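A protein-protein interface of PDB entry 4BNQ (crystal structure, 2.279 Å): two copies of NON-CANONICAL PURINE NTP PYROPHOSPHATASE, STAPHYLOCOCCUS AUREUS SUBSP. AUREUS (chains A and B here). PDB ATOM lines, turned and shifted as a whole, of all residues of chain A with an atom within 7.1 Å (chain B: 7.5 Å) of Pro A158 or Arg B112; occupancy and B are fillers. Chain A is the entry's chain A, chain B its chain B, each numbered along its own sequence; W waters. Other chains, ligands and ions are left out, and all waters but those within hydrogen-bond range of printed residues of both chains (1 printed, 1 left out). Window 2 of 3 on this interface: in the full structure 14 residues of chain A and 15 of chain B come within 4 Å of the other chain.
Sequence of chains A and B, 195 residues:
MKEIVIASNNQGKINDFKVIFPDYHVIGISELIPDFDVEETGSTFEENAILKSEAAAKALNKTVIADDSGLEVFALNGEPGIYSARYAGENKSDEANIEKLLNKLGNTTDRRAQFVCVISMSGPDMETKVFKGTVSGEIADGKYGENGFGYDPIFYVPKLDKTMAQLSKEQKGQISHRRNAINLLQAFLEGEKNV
The guanidinium group of Arg B112 is in hydrogen-bond range of the backbone carbonyl oxygen of Lys A159 (2.7 Å).
The backbone carbonyl oxygen of Arg B112 sits at hydrogen-bond distance from the backbone NH of Phe B74 (3.0 Å).
OD1 of Asp B110 is in salt-bridge range of NE of Arg B112 (2.9 Å).
Among the printed residues, pairs that only touch across the chains: Lys A159 with Ser B136, Ser A136 with Lys B159, Pro A158 with Arg B112 and Leu A160 with Arg B112.
Of the printed residues of chain B, Ser A136 touches Lys B159 (3.7 Å).
Pro A158 touches just one residue of chain B: Arg B112.
Of the printed residues of chain B, Lys A159 touches Arg B112 and Ser B136.
Printed residues of chain B within 4 Å of Leu A160: Arg B112.
Of chain A, only Pro A158 (3.8 Å), Lys A159 (2.7 Å) and Leu A160 (3.9 Å) come within 4 Å of Arg B112.
Printed residues of chain A within 4 Å of Ser B136: Lys A159.
The nearest residue of chain B that does not touch Pro A158 is Glu B138 (5.2 Å).
The nearest printed residue of chain A that does not touch Ser B136 is Ser A136 (4.9 Å).
Of the 11 printed residues of chain A, 4 touch a printed residue of chain B.
Of the 21 printed residues of chain B, 3 touch a printed residue of chain A.
Among the printed residues, 5 pairs touch across the chains.
Ser A136 touches Lys B159, and with the chains exchanged Lys A159 touches Ser B136.
Positions printed for both chains: 136, 137, 138, 155, 158 and 159.
Of the 5 pairs that touch across the chains among the printed residues, 2 have their exchanged pair printed and touching as well.
Water W1 bridges N of Ser B136 (3.5 Å) and NZ of Lys A159 (3.5 Å).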
ATOM      1  N   SER A 136      24.714   1.382 -17.696  1.00  0.00           N
ATOM      2  CA  SER A 136      23.703   0.684 -18.474  1.00  0.00           C
ATOM      3  C   SER A 136      24.082   0.624 -19.946  1.00  0.00           C
ATOM      4  O   SER A 136      24.836   1.471 -20.440  1.00  0.00           O
ATOM      5  CB  SER A 136      22.344   1.364 -18.324  1.00  0.00           C
ATOM      6  OG  SER A 136      22.357   2.660 -18.905  1.00  0.00           O
ATOM      7  N   GLY A 137      23.541  -0.379 -20.637  1.00  0.00           N
ATOM      8  CA  GLY A 137      23.747  -0.548 -22.061  1.00  0.00           C
ATOM      9  C   GLY A 137      22.878  -1.671 -22.603  1.00  0.00           C
ATOM     10  O   GLY A 137      21.896  -2.084 -21.973  1.00  0.00           O
ATOM     11  N   GLU A 138      23.250  -2.168 -23.777  1.00  0.00           N
ATOM     12  CA  GLU A 138      22.503  -3.208 -24.453  1.00  0.00           C
ATOM     13  C   GLU A 138      23.531  -4.168 -24.957  1.00  0.00           C
ATOM     14  O   GLU A 138      24.685  -3.776 -25.162  1.00  0.00           O
ATOM     15  CB  GLU A 138      21.728  -2.626 -25.641  1.00  0.00           C
ATOM     16  CG  GLU A 138      20.637  -1.642 -25.237  1.00  0.00           C
ATOM     17  CD  GLU A 138      19.902  -1.039 -26.428  1.00  0.00           C
ATOM     18  OE1 GLU A 138      20.556  -0.786 -27.466  1.00  0.00           O
ATOM     19  OE2 GLU A 138      18.673  -0.811 -26.324  1.00  0.00           O
ATOM     20  N   PHE A 155      29.197  -4.955 -25.346  1.00  0.00           N
ATOM     21  CA  PHE A 155      28.426  -4.066 -24.494  1.00  0.00           C
ATOM     22  C   PHE A 155      28.275  -2.680 -25.151  1.00  0.00           C
ATOM     23  O   PHE A 155      29.165  -1.824 -25.063  1.00  0.00           O
ATOM     24  CB  PHE A 155      29.059  -3.945 -23.103  1.00  0.00           C
ATOM     25  CG  PHE A 155      28.147  -3.316 -22.074  1.00  0.00           C
ATOM     26  CD1 PHE A 155      27.289  -4.100 -21.309  1.00  0.00           C
ATOM     27  CD2 PHE A 155      28.142  -1.946 -21.875  1.00  0.00           C
ATOM     28  CE1 PHE A 155      26.443  -3.521 -20.363  1.00  0.00           C
ATOM     29  CE2 PHE A 155      27.302  -1.363 -20.928  1.00  0.00           C
ATOM     30  CZ  PHE A 155      26.449  -2.154 -20.176  1.00  0.00           C
ATOM     31  N   TYR A 156      27.127  -2.476 -25.795  1.00  0.00           N
ATOM     32  CA  TYR A 156      26.832  -1.269 -26.548  1.00  0.00           C
ATOM     33  C   TYR A 156      26.315  -0.213 -25.587  1.00  0.00           C
ATOM     34  O   TYR A 156      25.431  -0.481 -24.762  1.00  0.00           O
ATOM     35  CB  TYR A 156      25.797  -1.583 -27.638  1.00  0.00           C
ATOM     36  CG  TYR A 156      25.316  -0.380 -28.403  1.00  0.00           C
ATOM     37  CD1 TYR A 156      26.070   0.157 -29.434  1.00  0.00           C
ATOM     38  CD2 TYR A 156      24.101   0.210 -28.103  1.00  0.00           C
ATOM     39  CE1 TYR A 156      25.634   1.272 -30.134  1.00  0.00           C
ATOM     40  CE2 TYR A 156      23.647   1.322 -28.803  1.00  0.00           C
ATOM     41  CZ  TYR A 156      24.420   1.847 -29.814  1.00  0.00           C
ATOM     42  OH  TYR A 156      23.982   2.934 -30.518  1.00  0.00           O
ATOM     43  N   VAL A 157      26.885   0.981 -25.674  1.00  0.00           N
ATOM     44  CA  VAL A 157      26.494   2.069 -24.782  1.00  0.00           C
ATOM     45  C   VAL A 157      25.747   3.134 -25.578  1.00  0.00           C
ATOM     46  O   VAL A 157      26.388   3.927 -26.274  1.00  0.00           O
ATOM     47  CB  VAL A 157      27.730   2.717 -24.120  1.00  0.00           C
ATOM     48  CG1 VAL A 157      27.306   3.783 -23.132  1.00  0.00           C
ATOM     49  CG2 VAL A 157      28.588   1.649 -23.410  1.00  0.00           C
ATOM     50  N   PRO A 158      24.398   3.147 -25.478  1.00  0.00           N
ATOM     51  CA  PRO A 158      23.539   4.039 -26.271  1.00  0.00           C
ATOM     52  C   PRO A 158      23.960   5.507 -26.177  1.00  0.00           C
ATOM     53  O   PRO A 158      24.064   6.145 -27.222  1.00  0.00           O
ATOM     54  CB  PRO A 158      22.146   3.831 -25.657  1.00  0.00           C
ATOM     55  CG  PRO A 158      22.190   2.439 -25.117  1.00  0.00           C
ATOM     56  CD  PRO A 158      23.599   2.330 -24.543  1.00  0.00           C
ATOM     57  N   LYS A 159      24.213   6.001 -24.963  1.00  0.00           N
ATOM     58  CA  LYS A 159      24.797   7.330 -24.704  1.00  0.00           C
ATOM     59  C   LYS A 159      25.894   7.702 -25.667  1.00  0.00           C
ATOM     60  O   LYS A 159      26.113   8.872 -25.938  1.00  0.00           O
ATOM     61  CB  LYS A 159      25.536   7.299 -23.364  1.00  0.00           C
ATOM     62  CG  LYS A 159      24.760   7.677 -22.160  1.00  0.00           C
ATOM     63  CD  LYS A 159      25.714   8.067 -21.029  1.00  0.00           C
ATOM     64  CE  LYS A 159      26.566   6.926 -20.550  1.00  0.00           C
ATOM     65  NZ  LYS A 159      26.902   7.115 -19.118  1.00  0.00           N
ATOM     66  N   LEU A 160      26.655   6.712 -26.114  1.00  0.00           N
ATOM     67  CA  LEU A 160      27.878   7.008 -26.848  1.00  0.00           C
ATOM     68  C   LEU A 160      27.782   6.488 -28.268  1.00  0.00           C
ATOM     69  O   LEU A 160      28.662   6.729 -29.081  1.00  0.00           O
ATOM     70  CB  LEU A 160      29.081   6.388 -26.130  1.00  0.00           C
ATOM     71  CG  LEU A 160      29.945   7.245 -25.189  1.00  0.00           C
ATOM     72  CD1 LEU A 160      29.120   8.224 -24.428  1.00  0.00           C
ATOM     73  CD2 LEU A 160      30.694   6.362 -24.210  1.00  0.00           C
ATOM     74  N   ASP A 161      26.692   5.778 -28.551  1.00  0.00           N
ATOM     75  CA  ASP A 161      26.545   5.002 -29.791  1.00  0.00           C
ATOM     76  C   ASP A 161      27.801   4.156 -30.097  1.00  0.00           C
ATOM     77  O   ASP A 161      28.253   4.095 -31.239  1.00  0.00           O
ATOM     78  CB  ASP A 161      26.210   5.928 -30.971  1.00  0.00           C
ATOM     79  CG  ASP A 161      25.778   5.161 -32.199  1.00  0.00           C
ATOM     80  OD1 ASP A 161      25.358   3.997 -32.055  1.00  0.00           O
ATOM     81  OD2 ASP A 161      25.862   5.710 -33.315  1.00  0.00           O
ATOM     82  N   LYS A 162      28.362   3.517 -29.071  1.00  0.00           N
ATOM     83  CA  LYS A 162      29.562   2.691 -29.228  1.00  0.00           C
ATOM     84  C   LYS A 162      29.545   1.547 -28.225  1.00  0.00           C
ATOM     85  O   LYS A 162      28.868   1.633 -27.199  1.00  0.00           O
ATOM     86  CB  LYS A 162      30.835   3.528 -29.025  1.00  0.00           C
ATOM     87  CG  LYS A 162      31.195   4.455 -30.187  1.00  0.00           C
ATOM     88  CD  LYS A 162      32.570   5.071 -29.981  1.00  0.00           C
ATOM     89  CE  LYS A 162      32.754   6.337 -30.811  1.00  0.00           C
ATOM     90  NZ  LYS A 162      32.349   6.120 -32.221  1.00  0.00           N
ATOM     91  N   LEU B  71      18.795  20.058 -17.301  1.00  0.00           N
ATOM     92  CA  LEU B  71      18.757  19.114 -18.387  1.00  0.00           C
ATOM     93  C   LEU B  71      19.717  19.604 -19.437  1.00  0.00           C
ATOM     94  O   LEU B  71      19.780  20.805 -19.719  1.00  0.00           O
ATOM     95  CB  LEU B  71      17.356  19.073 -18.973  1.00  0.00           C
ATOM     96  CG  LEU B  71      17.138  18.184 -20.194  1.00  0.00           C
ATOM     97  CD1 LEU B  71      17.363  16.727 -19.836  1.00  0.00           C
ATOM     98  CD2 LEU B  71      15.724  18.385 -20.753  1.00  0.00           C
ATOM     99  N   GLU B  72      20.489  18.689 -20.008  1.00  0.00           N
ATOM    100  CA  GLU B  72      21.340  19.031 -21.139  1.00  0.00           C
ATOM    101  C   GLU B  72      20.945  18.164 -22.310  1.00  0.00           C
ATOM    102  O   GLU B  72      20.958  16.943 -22.212  1.00  0.00           O
ATOM    103  CB  GLU B  72      22.819  18.840 -20.795  1.00  0.00           C
ATOM    104  CG  GLU B  72      23.324  19.824 -19.767  1.00  0.00           C
ATOM    105  CD  GLU B  72      24.746  19.545 -19.321  1.00  0.00           C
ATOM    106  OE1 GLU B  72      25.166  18.368 -19.337  1.00  0.00           O
ATOM    107  OE2 GLU B  72      25.439  20.508 -18.938  1.00  0.00           O
ATOM    108  N   VAL B  73      20.567  18.797 -23.410  1.00  0.00           N
ATOM    109  CA  VAL B  73      20.222  18.062 -24.617  1.00  0.00           C
ATOM    110  C   VAL B  73      21.339  18.233 -25.636  1.00  0.00           C
ATOM    111  O   VAL B  73      21.697  19.362 -25.995  1.00  0.00           O
ATOM    112  CB  VAL B  73      18.902  18.542 -25.196  1.00  0.00           C
ATOM    113  CG1 VAL B  73      18.625  17.827 -26.516  1.00  0.00           C
ATOM    114  CG2 VAL B  73      17.793  18.289 -24.193  1.00  0.00           C
ATOM    115  N   PHE B  74      21.889  17.108 -26.089  1.00  0.00           N
ATOM    116  CA  PHE B  74      23.126  17.105 -26.867  1.00  0.00           C
ATOM    117  C   PHE B  74      23.012  17.830 -28.204  1.00  0.00           C
ATOM    118  O   PHE B  74      23.927  18.557 -28.598  1.00  0.00           O
ATOM    119  CB  PHE B  74      23.634  15.667 -27.064  1.00  0.00           C
ATOM    120  CG  PHE B  74      24.796  15.556 -28.018  1.00  0.00           C
ATOM    121  CD1 PHE B  74      26.059  16.037 -27.665  1.00  0.00           C
ATOM    122  CD2 PHE B  74      24.629  14.961 -29.269  1.00  0.00           C
ATOM    123  CE1 PHE B  74      27.141  15.936 -28.550  1.00  0.00           C
ATOM    124  CE2 PHE B  74      25.701  14.861 -30.158  1.00  0.00           C
ATOM    125  CZ  PHE B  74      26.961  15.349 -29.795  1.00  0.00           C
ATOM    126  N   ALA B  75      21.894  17.631 -28.897  1.00  0.00           N
ATOM    127  CA  ALA B  75      21.680  18.293 -30.179  1.00  0.00           C
ATOM    128  C   ALA B  75      21.509  19.815 -30.050  1.00  0.00           C
ATOM    129  O   ALA B  75      21.774  20.552 -31.001  1.00  0.00           O
ATOM    130  CB  ALA B  75      20.498  17.674 -30.914  1.00  0.00           C
ATOM    131  N   LEU B  76      21.080  20.286 -28.880  1.00  0.00           N
ATOM    132  CA  LEU B  76      20.868  21.716 -28.666  1.00  0.00           C
ATOM    133  C   LEU B  76      22.096  22.356 -28.010  1.00  0.00           C
ATOM    134  O   LEU B  76      22.013  23.447 -27.442  1.00  0.00           O
ATOM    135  CB  LEU B  76      19.607  21.961 -27.825  1.00  0.00           C
ATOM    136  CG  LEU B  76      18.396  21.095 -28.180  1.00  0.00           C
ATOM    137  CD1 LEU B  76      17.189  21.405 -27.296  1.00  0.00           C
ATOM    138  CD2 LEU B  76      18.041  21.242 -29.649  1.00  0.00           C
ATOM    139  N   LEU B 105      13.896  21.094 -30.828  1.00  0.00           N
ATOM    140  CA  LEU B 105      14.483  19.813 -31.190  1.00  0.00           C
ATOM    141  C   LEU B 105      13.767  19.312 -32.429  1.00  0.00           C
ATOM    142  O   LEU B 105      14.361  19.209 -33.509  1.00  0.00           O
ATOM    143  CB  LEU B 105      14.321  18.815 -30.047  1.00  0.00           C
ATOM    144  CG  LEU B 105      15.167  17.545 -30.110  1.00  0.00           C
ATOM    145  CD1 LEU B 105      16.644  17.892 -30.183  1.00  0.00           C
ATOM    146  CD2 LEU B 105      14.871  16.692 -28.903  1.00  0.00           C
ATOM    147  N   THR B 108      14.713  16.367 -35.225  1.00  0.00           N
ATOM    148  CA  THR B 108      16.049  15.817 -34.972  1.00  0.00           C
ATOM    149  C   THR B 108      16.059  14.373 -34.434  1.00  0.00           C
ATOM    150  O   THR B 108      15.377  14.052 -33.459  1.00  0.00           O
ATOM    151  CB  THR B 108      16.848  16.741 -34.034  1.00  0.00           C
ATOM    152  OG1 THR B 108      16.544  18.111 -34.345  1.00  0.00           O
ATOM    153  CG2 THR B 108      18.353  16.489 -34.188  1.00  0.00           C
ATOM    154  N   THR B 109      16.846  13.518 -35.086  1.00  0.00           N
ATOM    155  CA  THR B 109      16.913  12.092 -34.767  1.00  0.00           C
ATOM    156  C   THR B 109      17.754  11.759 -33.519  1.00  0.00           C
ATOM    157  O   THR B 109      17.435  10.831 -32.770  1.00  0.00           O
ATOM    158  CB  THR B 109      17.457  11.301 -35.972  1.00  0.00           C
ATOM    159  OG1 THR B 109      17.645   9.932 -35.601  1.00  0.00           O
ATOM    160  CG2 THR B 109      18.796  11.874 -36.442  1.00  0.00           C
ATOM    161  N   ASP B 110      18.827  12.516 -33.314  1.00  0.00           N
ATOM    162  CA  ASP B 110      19.694  12.337 -32.155  1.00  0.00           C
ATOM    163  C   ASP B 110      19.092  13.082 -30.961  1.00  0.00           C
ATOM    164  O   ASP B 110      19.298  14.285 -30.805  1.00  0.00           O
ATOM    165  CB  ASP B 110      21.088  12.886 -32.469  1.00  0.00           C
ATOM    166  CG  ASP B 110      22.107  12.562 -31.391  1.00  0.00           C
ATOM    167  OD1 ASP B 110      21.719  12.055 -30.316  1.00  0.00           O
ATOM    168  OD2 ASP B 110      23.307  12.833 -31.616  1.00  0.00           O
ATOM    169  N   ARG B 111      18.351  12.368 -30.119  1.00  0.00           N
ATOM    170  CA  ARG B 111      17.640  13.001 -29.006  1.00  0.00           C
ATOM    171  C   ARG B 111      18.316  12.754 -27.647  1.00  0.00           C
ATOM    172  O   ARG B 111      17.699  12.927 -26.586  1.00  0.00           O
ATOM    173  CB  ARG B 111      16.179  12.546 -29.015  1.00  0.00           C
ATOM    174  CG  ARG B 111      15.542  12.804 -30.388  1.00  0.00           C
ATOM    175  CD  ARG B 111      14.101  12.338 -30.507  1.00  0.00           C
ATOM    176  NE  ARG B 111      13.157  13.247 -29.865  1.00  0.00           N
ATOM    177  CZ  ARG B 111      12.769  14.414 -30.370  1.00  0.00           C
ATOM    178  NH1 ARG B 111      13.258  14.846 -31.526  1.00  0.00           N
ATOM    179  NH2 ARG B 111      11.901  15.160 -29.703  1.00  0.00           N
ATOM    180  N   ARG B 112      19.592  12.369 -27.700  1.00  0.00           N
ATOM    181  CA  ARG B 112      20.357  12.056 -26.497  1.00  0.00           C
ATOM    182  C   ARG B 112      20.434  13.244 -25.554  1.00  0.00           C
ATOM    183  O   ARG B 112      20.627  14.392 -25.981  1.00  0.00           O
ATOM    184  CB  ARG B 112      21.764  11.571 -26.855  1.00  0.00           C
ATOM    185  CG  ARG B 112      21.789  10.168 -27.436  1.00  0.00           C
ATOM    186  CD  ARG B 112      23.183   9.781 -27.835  1.00  0.00           C
ATOM    187  NE  ARG B 112      23.793  10.791 -28.695  1.00  0.00           N
ATOM    188  CZ  ARG B 112      25.093  10.850 -28.962  1.00  0.00           C
ATOM    189  NH1 ARG B 112      25.920   9.958 -28.433  1.00  0.00           N
ATOM    190  NH2 ARG B 112      25.566  11.801 -29.751  1.00  0.00           N
ATOM    191  N   ALA B 113      20.265  12.962 -24.266  1.00  0.00           N
ATOM    192  CA  ALA B 113      20.278  14.017 -23.256  1.00  0.00           C
ATOM    193  C   ALA B 113      20.645  13.439 -21.887  1.00  0.00           C
ATOM    194  O   ALA B 113      20.584  12.214 -21.681  1.00  0.00           O
ATOM    195  CB  ALA B 113      18.916  14.703 -23.204  1.00  0.00           C
ATOM    196  N   GLN B 114      21.010  14.317 -20.954  1.00  0.00           N
ATOM    197  CA  GLN B 114      21.292  13.903 -19.578  1.00  0.00           C
ATOM    198  C   GLN B 114      20.794  14.928 -18.555  1.00  0.00           C
ATOM    199  O   GLN B 114      20.808  16.136 -18.809  1.00  0.00           O
ATOM    200  CB  GLN B 114      22.798  13.669 -19.380  1.00  0.00           C
ATOM    201  CG  GLN B 114      23.646  14.926 -19.545  1.00  0.00           C
ATOM    202  CD  GLN B 114      25.129  14.691 -19.284  1.00  0.00           C
ATOM    203  OE1 GLN B 114      25.548  13.580 -18.945  1.00  0.00           O
ATOM    204  NE2 GLN B 114      25.929  15.744 -19.438  1.00  0.00           N
ATOM    205  N   SER B 136      21.452   9.426 -17.770  1.00  0.00           N
ATOM    206  CA  SER B 136      21.337   9.639 -19.206  1.00  0.00           C
ATOM    207  C   SER B 136      19.998   9.160 -19.734  1.00  0.00           C
ATOM    208  O   SER B 136      19.364   8.294 -19.128  1.00  0.00           O
ATOM    209  CB  SER B 136      22.467   8.942 -19.957  1.00  0.00           C
ATOM    210  OG  SER B 136      22.417   7.527 -19.793  1.00  0.00           O
ATOM    211  N   GLY B 137      19.573   9.740 -20.856  1.00  0.00           N
ATOM    212  CA  GLY B 137      18.373   9.300 -21.546  1.00  0.00           C
ATOM    213  C   GLY B 137      18.153   9.997 -22.880  1.00  0.00           C
ATOM    214  O   GLY B 137      19.081  10.570 -23.466  1.00  0.00           O
ATOM    215  N   GLU B 138      16.919   9.941 -23.371  1.00  0.00           N
ATOM    216  CA  GLU B 138      16.582  10.538 -24.659  1.00  0.00           C
ATOM    217  C   GLU B 138      15.319  11.377 -24.519  1.00  0.00           C
ATOM    218  O   GLU B 138      14.381  10.982 -23.813  1.00  0.00           O
ATOM    219  CB  GLU B 138      16.329   9.452 -25.717  1.00  0.00           C
ATOM    220  CG  GLU B 138      17.463   8.485 -26.000  1.00  0.00           C
ATOM    221  CD  GLU B 138      17.034   7.317 -26.903  1.00  0.00           C
ATOM    222  OE1 GLU B 138      15.858   7.278 -27.336  1.00  0.00           O
ATOM    223  OE2 GLU B 138      17.868   6.424 -27.174  1.00  0.00           O
ATOM    224  N   ILE B 139      15.288  12.513 -25.206  1.00  0.00           N
ATOM    225  CA  ILE B 139      14.067  13.308 -25.276  1.00  0.00           C
ATOM    226  C   ILE B 139      12.998  12.546 -26.062  1.00  0.00           C
ATOM    227  O   ILE B 139      13.233  12.133 -27.199  1.00  0.00           O
ATOM    228  CB  ILE B 139      14.298  14.651 -25.957  1.00  0.00           C
ATOM    229  CG1 ILE B 139      15.394  15.427 -25.233  1.00  0.00           C
ATOM    230  CG2 ILE B 139      13.010  15.438 -25.992  1.00  0.00           C
ATOM    231  CD1 ILE B 139      15.222  15.461 -23.722  1.00  0.00           C
ATOM    232  N   PHE B 155      11.580  13.005 -20.683  1.00  0.00           N
ATOM    233  CA  PHE B 155      12.897  12.398 -20.505  1.00  0.00           C
ATOM    234  C   PHE B 155      12.781  10.881 -20.427  1.00  0.00           C
ATOM    235  O   PHE B 155      12.495  10.325 -19.367  1.00  0.00           O
ATOM    236  CB  PHE B 155      13.586  12.928 -19.250  1.00  0.00           C
ATOM    237  CG  PHE B 155      15.047  12.591 -19.178  1.00  0.00           C
ATOM    238  CD1 PHE B 155      15.989  13.421 -19.765  1.00  0.00           C
ATOM    239  CD2 PHE B 155      15.482  11.445 -18.536  1.00  0.00           C
ATOM    240  CE1 PHE B 155      17.352  13.114 -19.706  1.00  0.00           C
ATOM    241  CE2 PHE B 155      16.839  11.127 -18.476  1.00  0.00           C
ATOM    242  CZ  PHE B 155      17.775  11.964 -19.066  1.00  0.00           C
ATOM    243  N   PRO B 158      15.923   4.686 -21.248  1.00  0.00           N
ATOM    244  CA  PRO B 158      16.079   3.415 -21.962  1.00  0.00           C
ATOM    245  C   PRO B 158      16.198   2.220 -21.040  1.00  0.00           C
ATOM    246  O   PRO B 158      15.472   1.241 -21.237  1.00  0.00           O
ATOM    247  CB  PRO B 158      17.371   3.619 -22.742  1.00  0.00           C
ATOM    248  CG  PRO B 158      17.308   5.096 -23.110  1.00  0.00           C
ATOM    249  CD  PRO B 158      16.730   5.757 -21.869  1.00  0.00           C
ATOM    250  N   LYS B 159      17.060   2.297 -20.032  1.00  0.00           N
ATOM    251  CA  LYS B 159      17.239   1.165 -19.121  1.00  0.00           C
ATOM    252  C   LYS B 159      15.971   0.793 -18.346  1.00  0.00           C
ATOM    253  O   LYS B 159      15.907  -0.257 -17.715  1.00  0.00           O
ATOM    254  CB  LYS B 159      18.403   1.407 -18.151  1.00  0.00           C
ATOM    255  CG  LYS B 159      18.198   2.550 -17.150  1.00  0.00           C
ATOM    256  CD  LYS B 159      19.491   2.771 -16.342  1.00  0.00           C
ATOM    257  CE  LYS B 159      19.378   3.918 -15.348  1.00  0.00           C
ATOM    258  NZ  LYS B 159      20.636   4.017 -14.558  1.00  0.00           N
HETATM  259  O   HOH W   1      24.886   9.242 -17.207  1.00  0.00           O
